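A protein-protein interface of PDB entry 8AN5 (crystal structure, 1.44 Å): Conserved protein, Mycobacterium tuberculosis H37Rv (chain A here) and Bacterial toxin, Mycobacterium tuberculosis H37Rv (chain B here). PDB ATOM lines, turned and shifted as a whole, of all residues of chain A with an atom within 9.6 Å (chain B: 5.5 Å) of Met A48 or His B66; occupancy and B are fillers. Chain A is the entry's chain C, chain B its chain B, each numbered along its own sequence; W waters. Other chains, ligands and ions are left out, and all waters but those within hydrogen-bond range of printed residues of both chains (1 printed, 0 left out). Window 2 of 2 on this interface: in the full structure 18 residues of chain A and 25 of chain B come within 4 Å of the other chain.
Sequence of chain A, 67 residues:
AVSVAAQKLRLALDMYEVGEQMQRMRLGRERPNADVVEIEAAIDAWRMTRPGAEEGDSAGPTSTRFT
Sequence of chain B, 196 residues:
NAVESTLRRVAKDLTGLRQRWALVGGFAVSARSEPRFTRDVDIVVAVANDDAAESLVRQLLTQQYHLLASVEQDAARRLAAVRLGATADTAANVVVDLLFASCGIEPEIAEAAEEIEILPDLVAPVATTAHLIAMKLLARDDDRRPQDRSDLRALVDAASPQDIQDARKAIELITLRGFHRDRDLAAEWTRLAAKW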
ATOM      1  N   TYR A  16      -5.610 -35.405  19.724  1.00  0.00           N
ATOM      2  CA  TYR A  16      -5.294 -34.392  20.739  1.00  0.00           C
ATOM      3  C   TYR A  16      -4.198 -34.933  21.660  1.00  0.00           C
ATOM      4  O   TYR A  16      -3.289 -34.252  21.924  1.00  0.00           O
ATOM      5  CB  TYR A  16      -6.510 -33.975  21.592  1.00  0.00           C
ATOM      6  CG  TYR A  16      -6.025 -33.224  22.788  1.00  0.00           C
ATOM      7  CD1 TYR A  16      -5.652 -31.913  22.676  1.00  0.00           C
ATOM      8  CD2 TYR A  16      -5.772 -33.860  23.969  1.00  0.00           C
ATOM      9  CE1 TYR A  16      -5.057 -31.253  23.713  1.00  0.00           C
ATOM     10  CE2 TYR A  16      -5.178 -33.215  25.017  1.00  0.00           C
ATOM     11  CZ  TYR A  16      -4.830 -31.900  24.897  1.00  0.00           C
ATOM     12  OH  TYR A  16      -4.230 -31.258  25.911  1.00  0.00           O
ATOM     13  N   GLU A  40       4.962 -28.984  32.696  1.00  0.00           N
ATOM     14  CA  GLU A  40       3.516 -29.145  32.806  1.00  0.00           C
ATOM     15  C   GLU A  40       2.832 -27.794  32.933  1.00  0.00           C
ATOM     16  O   GLU A  40       1.743 -27.586  32.384  1.00  0.00           O
ATOM     17  CB  GLU A  40       3.166 -30.032  33.996  1.00  0.00           C
ATOM     18  CG  GLU A  40       3.318 -31.525  33.745  1.00  0.00           C
ATOM     19  CD  GLU A  40       2.831 -31.956  32.364  1.00  0.00           C
ATOM     20  OE1 GLU A  40       3.685 -32.260  31.506  1.00  0.00           O
ATOM     21  OE2 GLU A  40       1.602 -31.974  32.132  1.00  0.00           O
ATOM     22  N   ALA A  41       3.449 -26.865  33.672  1.00  0.00           N
ATOM     23  CA  ALA A  41       2.936 -25.501  33.724  1.00  0.00           C
ATOM     24  C   ALA A  41       2.899 -24.886  32.333  1.00  0.00           C
ATOM     25  O   ALA A  41       1.932 -24.207  31.969  1.00  0.00           O
ATOM     26  CB  ALA A  41       3.802 -24.650  34.661  1.00  0.00           C
ATOM     27  N   ALA A  42       3.947 -25.104  31.544  1.00  0.00           N
ATOM     28  CA  ALA A  42       3.934 -24.617  30.170  1.00  0.00           C
ATOM     29  C   ALA A  42       2.851 -25.311  29.350  1.00  0.00           C
ATOM     30  O   ALA A  42       2.221 -24.684  28.492  1.00  0.00           O
ATOM     31  CB  ALA A  42       5.310 -24.800  29.534  1.00  0.00           C
ATOM     32  N   ILE A  43       2.629 -26.607  29.587  1.00  0.00           N
ATOM     33  CA  ILE A  43       1.585 -27.315  28.855  1.00  0.00           C
ATOM     34  C   ILE A  43       0.214 -26.743  29.201  1.00  0.00           C
ATOM     35  O   ILE A  43      -0.630 -26.547  28.321  1.00  0.00           O
ATOM     36  CB  ILE A  43       1.675 -28.829  29.117  1.00  0.00           C
ATOM     37  CG1 ILE A  43       2.842 -29.437  28.336  1.00  0.00           C
ATOM     38  CG2 ILE A  43       0.399 -29.518  28.693  1.00  0.00           C
ATOM     39  CD1 ILE A  43       2.665 -29.368  26.829  1.00  0.00           C
ATOM     40  N   ASP A  44       0.019 -26.412  30.469  1.00  0.00           N
ATOM     41  CA  ASP A  44      -1.265 -25.852  30.937  1.00  0.00           C
ATOM     42  C   ASP A  44      -1.491 -24.477  30.347  1.00  0.00           C
ATOM     43  O   ASP A  44      -2.547 -24.227  29.828  1.00  0.00           O
ATOM     44  CB  ASP A  44      -1.381 -25.927  32.448  1.00  0.00           C
ATOM     45  CG  ASP A  44      -2.816 -25.673  32.801  1.00  0.00           C
ATOM     46  OD1 ASP A  44      -3.587 -26.636  32.820  1.00  0.00           O
ATOM     47  OD2 ASP A  44      -3.151 -24.508  32.931  1.00  0.00           O
ATOM     48  N   ALA A  45      -0.464 -23.666  30.249  1.00  0.00           N
ATOM     49  CA  ALA A  45      -0.579 -22.334  29.645  1.00  0.00           C
ATOM     50  C   ALA A  45      -0.955 -22.473  28.182  1.00  0.00           C
ATOM     51  O   ALA A  45      -1.679 -21.657  27.677  1.00  0.00           O
ATOM     52  CB  ALA A  45       0.702 -21.580  29.787  1.00  0.00           C
ATOM     53  N   TRP A  46      -0.433 -23.506  27.547  1.00  0.00           N
ATOM     54  CA  TRP A  46      -0.602 -23.749  26.101  1.00  0.00           C
ATOM     55  C   TRP A  46      -2.080 -23.936  25.765  1.00  0.00           C
ATOM     56  O   TRP A  46      -2.565 -23.341  24.852  1.00  0.00           O
ATOM     57  CB  TRP A  46       0.260 -24.956  25.726  1.00  0.00           C
ATOM     58  CG  TRP A  46      -0.081 -25.586  24.425  1.00  0.00           C
ATOM     59  CD1 TRP A  46       0.019 -24.996  23.227  1.00  0.00           C
ATOM     60  CD2 TRP A  46      -0.571 -26.911  24.173  1.00  0.00           C
ATOM     61  NE1 TRP A  46      -0.457 -25.847  22.297  1.00  0.00           N
ATOM     62  CE2 TRP A  46      -0.713 -27.038  22.789  1.00  0.00           C
ATOM     63  CE3 TRP A  46      -0.904 -28.009  24.937  1.00  0.00           C
ATOM     64  CZ2 TRP A  46      -1.185 -28.151  22.140  1.00  0.00           C
ATOM     65  CZ3 TRP A  46      -1.370 -29.130  24.312  1.00  0.00           C
ATOM     66  CH2 TRP A  46      -1.493 -29.205  22.931  1.00  0.00           C
ATOM     67  N   ARG A  47      -2.756 -24.819  26.466  1.00  0.00           N
ATOM     68  CA  ARG A  47      -4.201 -25.032  26.239  1.00  0.00           C
ATOM     69  C   ARG A  47      -4.954 -23.705  26.383  1.00  0.00           C
ATOM     70  O   ARG A  47      -5.743 -23.348  25.531  1.00  0.00           O
ATOM     71  CB  ARG A  47      -4.760 -25.981  27.294  1.00  0.00           C
ATOM     72  CG  ARG A  47      -4.325 -27.437  27.179  1.00  0.00           C
ATOM     73  CD  ARG A  47      -3.749 -27.936  28.489  1.00  0.00           C
ATOM     74  NE  ARG A  47      -3.664 -29.377  28.651  1.00  0.00           N
ATOM     75  CZ  ARG A  47      -3.242 -30.014  29.752  1.00  0.00           C
ATOM     76  NH1 ARG A  47      -2.854 -29.357  30.838  1.00  0.00           N
ATOM     77  NH2 ARG A  47      -3.204 -31.335  29.767  1.00  0.00           N
ATOM     78  N   MET A  48      -4.648 -22.909  27.378  1.00  0.00           N
ATOM     79  CA  MET A  48      -5.449 -21.716  27.703  1.00  0.00           C
ATOM     80  C   MET A  48      -5.360 -20.667  26.608  1.00  0.00           C
ATOM     81  O   MET A  48      -6.229 -19.837  26.520  1.00  0.00           O
ATOM     82  CB  MET A  48      -4.953 -21.110  29.002  1.00  0.00           C
ATOM     83  CG  MET A  48      -5.371 -21.824  30.234  1.00  0.00           C
ATOM     84  SD  MET A  48      -5.065 -20.598  31.521  1.00  0.00           S
ATOM     85  CE  MET A  48      -5.948 -21.248  32.936  1.00  0.00           C
ATOM     86  N   THR A  49      -4.319 -20.663  25.821  1.00  0.00           N
ATOM     87  CA  THR A  49      -4.154 -19.660  24.769  1.00  0.00           C
ATOM     88  C   THR A  49      -5.122 -19.969  23.626  1.00  0.00           C
ATOM     89  O   THR A  49      -5.226 -21.108  23.290  1.00  0.00           O
ATOM     90  CB  THR A  49      -2.672 -19.660  24.393  1.00  0.00           C
ATOM     91  OG1 THR A  49      -1.902 -19.747  25.590  1.00  0.00           O
ATOM     92  CG2 THR A  49      -2.246 -18.433  23.637  1.00  0.00           C
ATOM     93  N   ARG A  50      -5.660 -18.957  22.921  1.00  0.00           N
ATOM     94  CA  ARG A  50      -6.549 -19.096  21.755  1.00  0.00           C
ATOM     95  C   ARG A  50      -5.822 -19.692  20.550  1.00  0.00           C
ATOM     96  O   ARG A  50      -4.589 -19.798  20.567  1.00  0.00           O
ATOM     97  CB  ARG A  50      -7.142 -17.738  21.357  1.00  0.00           C
ATOM     98  CG  ARG A  50      -8.214 -17.197  22.296  1.00  0.00           C
ATOM     99  CD  ARG A  50      -8.759 -15.859  21.798  1.00  0.00           C
ATOM    100  NE  ARG A  50      -9.745 -15.289  22.715  1.00  0.00           N
ATOM    101  CZ  ARG A  50     -10.338 -14.109  22.548  1.00  0.00           C
ATOM    102  NH1 ARG A  50     -10.054 -13.360  21.489  1.00  0.00           N
ATOM    103  NH2 ARG A  50     -11.222 -13.679  23.441  1.00  0.00           N
ATOM    104  N   PRO A  51      -6.545 -20.091  19.481  1.00  0.00           N
ATOM    105  CA  PRO A  51      -5.882 -20.655  18.297  1.00  0.00           C
ATOM    106  C   PRO A  51      -4.703 -19.820  17.812  1.00  0.00           C
ATOM    107  O   PRO A  51      -3.570 -20.120  18.191  1.00  0.00           O
ATOM    108  CB  PRO A  51      -6.993 -20.654  17.240  1.00  0.00           C
ATOM    109  CG  PRO A  51      -8.254 -20.781  18.021  1.00  0.00           C
ATOM    110  CD  PRO A  51      -8.014 -20.058  19.330  1.00  0.00           C
ATOM    111  N   ARG B  39      -7.604 -28.670  19.934  1.00  0.00           N
ATOM    112  CA  ARG B  39      -7.462 -28.608  21.382  1.00  0.00           C
ATOM    113  C   ARG B  39      -8.512 -27.793  22.088  1.00  0.00           C
ATOM    114  O   ARG B  39      -8.675 -27.963  23.303  1.00  0.00           O
ATOM    115  CB  ARG B  39      -6.063 -28.129  21.783  1.00  0.00           C
ATOM    116  CG  ARG B  39      -5.638 -26.851  21.162  1.00  0.00           C
ATOM    117  CD  ARG B  39      -4.241 -26.582  21.663  1.00  0.00           C
ATOM    118  NE  ARG B  39      -3.709 -25.317  21.201  1.00  0.00           N
ATOM    119  CZ  ARG B  39      -4.051 -24.143  21.712  1.00  0.00           C
ATOM    120  NH1 ARG B  39      -4.936 -24.087  22.696  1.00  0.00           N
ATOM    121  NH2 ARG B  39      -3.509 -23.029  21.238  1.00  0.00           N
ATOM    122  N   LEU B  61     -19.445 -20.902  37.176  1.00  0.00           N
ATOM    123  CA  LEU B  61     -18.352 -20.465  38.037  1.00  0.00           C
ATOM    124  C   LEU B  61     -18.456 -21.073  39.437  1.00  0.00           C
ATOM    125  O   LEU B  61     -17.435 -21.183  40.123  1.00  0.00           O
ATOM    126  CB  LEU B  61     -18.302 -18.937  38.066  1.00  0.00           C
ATOM    127  CG  LEU B  61     -18.051 -18.268  36.711  1.00  0.00           C
ATOM    128  CD1 LEU B  61     -17.854 -16.791  36.870  1.00  0.00           C
ATOM    129  CD2 LEU B  61     -16.858 -18.871  36.010  1.00  0.00           C
ATOM    130  N   GLN B  64     -16.634 -25.033  39.558  1.00  0.00           N
ATOM    131  CA  GLN B  64     -15.210 -25.241  39.323  1.00  0.00           C
ATOM    132  C   GLN B  64     -14.803 -24.921  37.887  1.00  0.00           C
ATOM    133  O   GLN B  64     -13.909 -25.556  37.328  1.00  0.00           O
ATOM    134  CB  GLN B  64     -14.778 -26.652  39.741  1.00  0.00           C
ATOM    135  CG  GLN B  64     -15.165 -26.986  41.197  1.00  0.00           C
ATOM    136  CD  GLN B  64     -14.698 -28.361  41.653  1.00  0.00           C
ATOM    137  OE1 GLN B  64     -13.857 -28.994  41.011  1.00  0.00           O
ATOM    138  NE2 GLN B  64     -15.238 -28.827  42.779  1.00  0.00           N
ATOM    139  N   TYR B  65     -15.461 -23.947  37.277  1.00  0.00           N
ATOM    140  CA  TYR B  65     -14.952 -23.283  36.091  1.00  0.00           C
ATOM    141  C   TYR B  65     -14.525 -21.877  36.486  1.00  0.00           C
ATOM    142  O   TYR B  65     -15.029 -21.304  37.451  1.00  0.00           O
ATOM    143  CB  TYR B  65     -16.023 -23.172  35.003  1.00  0.00           C
ATOM    144  CG  TYR B  65     -16.527 -24.491  34.475  1.00  0.00           C
ATOM    145  CD1 TYR B  65     -17.545 -25.177  35.127  1.00  0.00           C
ATOM    146  CD2 TYR B  65     -15.979 -25.057  33.331  1.00  0.00           C
ATOM    147  CE1 TYR B  65     -18.011 -26.404  34.644  1.00  0.00           C
ATOM    148  CE2 TYR B  65     -16.446 -26.266  32.833  1.00  0.00           C
ATOM    149  CZ  TYR B  65     -17.458 -26.931  33.490  1.00  0.00           C
ATOM    150  OH  TYR B  65     -17.898 -28.129  33.008  1.00  0.00           O
ATOM    151  N   HIS B  66     -13.572 -21.326  35.755  1.00  0.00           N
ATOM    152  CA  HIS B  66     -13.191 -19.940  35.955  1.00  0.00           C
ATOM    153  C   HIS B  66     -13.237 -19.243  34.612  1.00  0.00           C
ATOM    154  O   HIS B  66     -13.146 -19.874  33.554  1.00  0.00           O
ATOM    155  CB  HIS B  66     -11.862 -19.745  36.694  1.00  0.00           C
ATOM    156  CG  HIS B  66     -10.671 -20.285  35.977  1.00  0.00           C
ATOM    157  ND1 HIS B  66     -10.398 -21.633  35.901  1.00  0.00           N
ATOM    158  CD2 HIS B  66      -9.671 -19.658  35.315  1.00  0.00           C
ATOM    159  CE1 HIS B  66      -9.284 -21.817  35.215  1.00  0.00           C
ATOM    160  NE2 HIS B  66      -8.820 -20.633  34.850  1.00  0.00           N
ATOM    161  N   LEU B  67     -13.446 -17.942  34.667  1.00  0.00           N
ATOM    162  CA  LEU B  67     -13.675 -17.152  33.469  1.00  0.00           C
ATOM    163  C   LEU B  67     -12.323 -16.707  32.931  1.00  0.00           C
ATOM    164  O   LEU B  67     -11.619 -15.935  33.580  1.00  0.00           O
ATOM    165  CB  LEU B  67     -14.557 -15.956  33.797  1.00  0.00           C
ATOM    166  CG  LEU B  67     -14.921 -15.082  32.598  1.00  0.00           C
ATOM    167  CD1 LEU B  67     -15.727 -15.832  31.564  1.00  0.00           C
ATOM    168  CD2 LEU B  67     -15.663 -13.849  33.076  1.00  0.00           C
ATOM    169  N   LEU B  68     -11.968 -17.180  31.741  1.00  0.00           N
ATOM    170  CA  LEU B  68     -10.718 -16.760  31.124  1.00  0.00           C
ATOM    171  C   LEU B  68     -10.899 -15.513  30.273  1.00  0.00           C
ATOM    172  O   LEU B  68     -10.025 -14.642  30.258  1.00  0.00           O
ATOM    173  CB  LEU B  68     -10.155 -17.885  30.252  1.00  0.00           C
ATOM    174  CG  LEU B  68      -9.711 -19.165  30.951  1.00  0.00           C
ATOM    175  CD1 LEU B  68      -9.375 -20.232  29.912  1.00  0.00           C
ATOM    176  CD2 LEU B  68      -8.528 -18.900  31.852  1.00  0.00           C
ATOM    177  N   ARG B  83     -15.010 -17.807  27.423  1.00  0.00           N
ATOM    178  CA  ARG B  83     -13.944 -18.800  27.379  1.00  0.00           C
ATOM    179  C   ARG B  83     -13.752 -19.214  28.834  1.00  0.00           C
ATOM    180  O   ARG B  83     -13.464 -18.375  29.621  1.00  0.00           O
ATOM    181  CB  ARG B  83     -12.690 -18.215  26.730  1.00  0.00           C
ATOM    182  CG  ARG B  83     -11.564 -19.214  26.611  1.00  0.00           C
ATOM    183  CD  ARG B  83     -10.385 -18.757  25.796  1.00  0.00           C
ATOM    184  NE  ARG B  83     -10.903 -18.406  24.512  1.00  0.00           N
ATOM    185  CZ  ARG B  83     -10.635 -19.040  23.384  1.00  0.00           C
ATOM    186  NH1 ARG B  83     -11.210 -18.627  22.268  1.00  0.00           N
ATOM    187  NH2 ARG B  83      -9.831 -20.094  23.373  1.00  0.00           N
ATOM    188  N   LEU B  84     -13.936 -20.461  29.168  1.00  0.00           N
ATOM    189  CA  LEU B  84     -13.847 -20.938  30.536  1.00  0.00           C
ATOM    190  C   LEU B  84     -12.723 -21.956  30.656  1.00  0.00           C
ATOM    191  O   LEU B  84     -12.484 -22.742  29.744  1.00  0.00           O
ATOM    192  CB  LEU B  84     -15.128 -21.648  30.928  1.00  0.00           C
ATOM    193  CG  LEU B  84     -16.424 -20.847  30.870  1.00  0.00           C
ATOM    194  CD1 LEU B  84     -17.616 -21.703  31.265  1.00  0.00           C
ATOM    195  CD2 LEU B  84     -16.291 -19.612  31.778  1.00  0.00           C
ATOM    196  N   GLY B  85     -12.066 -21.985  31.801  1.00  0.00           N
ATOM    197  CA  GLY B  85     -11.059 -22.988  32.081  1.00  0.00           C
ATOM    198  C   GLY B  85     -11.515 -23.891  33.208  1.00  0.00           C
ATOM    199  O   GLY B  85     -12.332 -23.496  34.039  1.00  0.00           O
ATOM    200  N   ALA B  86     -11.000 -25.119  33.211  1.00  0.00           N
ATOM    201  CA  ALA B  86     -11.156 -26.006  34.358  1.00  0.00           C
ATOM    202  C   ALA B  86     -10.248 -25.551  35.499  1.00  0.00           C
ATOM    203  O   ALA B  86      -9.104 -25.141  35.279  1.00  0.00           O
ATOM    204  CB  ALA B  86     -10.797 -27.439  33.957  1.00  0.00           C
ATOM    205  N   THR B  87     -10.761 -25.614  36.723  1.00  0.00           N
ATOM    206  CA  THR B  87      -9.980 -25.205  37.889  1.00  0.00           C
ATOM    207  C   THR B  87      -9.220 -26.380  38.499  1.00  0.00           C
ATOM    208  O   THR B  87      -9.180 -27.471  37.932  1.00  0.00           O
ATOM    209  CB  THR B  87     -10.857 -24.560  38.985  1.00  0.00           C
ATOM    210  OG1 THR B  87     -11.853 -25.494  39.419  1.00  0.00           O
ATOM    211  CG2 THR B  87     -11.531 -23.301  38.473  1.00  0.00           C
ATOM    212  N   VAL B  95      -9.534 -25.561  27.835  1.00  0.00           N
ATOM    213  CA  VAL B  95     -10.457 -24.485  27.504  1.00  0.00           C
ATOM    214  C   VAL B  95     -11.766 -24.991  26.935  1.00  0.00           C
ATOM    215  O   VAL B  95     -11.796 -25.842  26.042  1.00  0.00           O
ATOM    216  CB  VAL B  95      -9.795 -23.558  26.477  1.00  0.00           C
ATOM    217  CG1 VAL B  95     -10.779 -22.619  25.882  1.00  0.00           C
ATOM    218  CG2 VAL B  95      -8.749 -22.719  27.146  1.00  0.00           C
HETATM  219  O   HOH W   1      -6.752 -25.324  24.338  1.00  0.00           O
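The guanidinium group (NH2) of Arg B39 sits at hydrogen-bond distance from the backbone carbonyl oxygen (O) of Arg A50 (3.5 Å).
NH1 of Arg B39 is in hydrogen-bond range of O of Arg A47.
The backbone carbonyl oxygen (O) of Trp A46 sits at hydrogen-bond distance from the guanidinium group (NH1) of Arg B39 (3.3 Å).
NH1 of Arg B39 lies within hydrogen-bond range of O of Thr A49.
O of Arg B83 is in hydrogen-bond range of N of Leu B68, at 2.9 Å.
NH1 of Arg A47 lies within salt-bridge range of OD1 of Asp A44 (3.4 Å).
The side-chain hydroxyl (OH) of Tyr A16 sits at hydrogen-bond distance from the guanidinium group (NE) of Arg A47, 3.4 Å away.
The backbone carbonyl oxygen of His B66 sits at hydrogen-bond distance from the backbone NH of Gly B85 (2.9 Å).
The side-chain hydroxyl (OG1) of Thr A49 lies within hydrogen-bond range of the backbone carbonyl oxygen (O) of Ala A45, at 2.8 Å.
Among the printed residues, pairs that only touch across the chains: Tyr A16 with Arg B39 (3.8 Å), Arg A47 with Val B95 (3.5 Å), Met A48 with His B66 (3.5 Å), Met A48 with Leu B68 (3.7 Å), Met A48 with Val B95 (3.5 Å) and Arg A50 with Arg B83 (3.2 Å).
Of the printed residues of chain B, Tyr A16 touches Arg B39 (3.8 Å).
Ala A45 touches none of the printed residues of chain B.
Of the printed residues of chain B, Arg A47 touches Arg B39 (3.0 Å) and Val B95 (3.5 Å).
Met A48 touches just these residues of chain B: His B66, Leu B68 and Val B95.
Of the printed residues of chain B, Thr A49 touches Arg B39.
His B66 touches one residue of chain A.
No residue of chain A comes within 4 Å of Gly B85.
The nearest residue of chain B that does not touch Met A48 is Arg B83 (4.4 Å).
The nearest residue of chain A that does not touch His B66 is Asp A44 (7.1 Å).
Of the 13 printed residues of chain A, 6 touch a printed residue of chain B.
Printed residues of chain A that touch a printed residue of chain B: Tyr A16, Trp A46, Arg A47, Met A48, Thr A49 and Arg A50.
Printed residues of chain B that touch a printed residue of chain A: Arg B39, His B66, Leu B68, Arg B83 and Val B95.
Among the printed residues, 10 pairs touch across the chains.
Water W1 bridges O of Arg A47 and NH1 of Arg B39.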
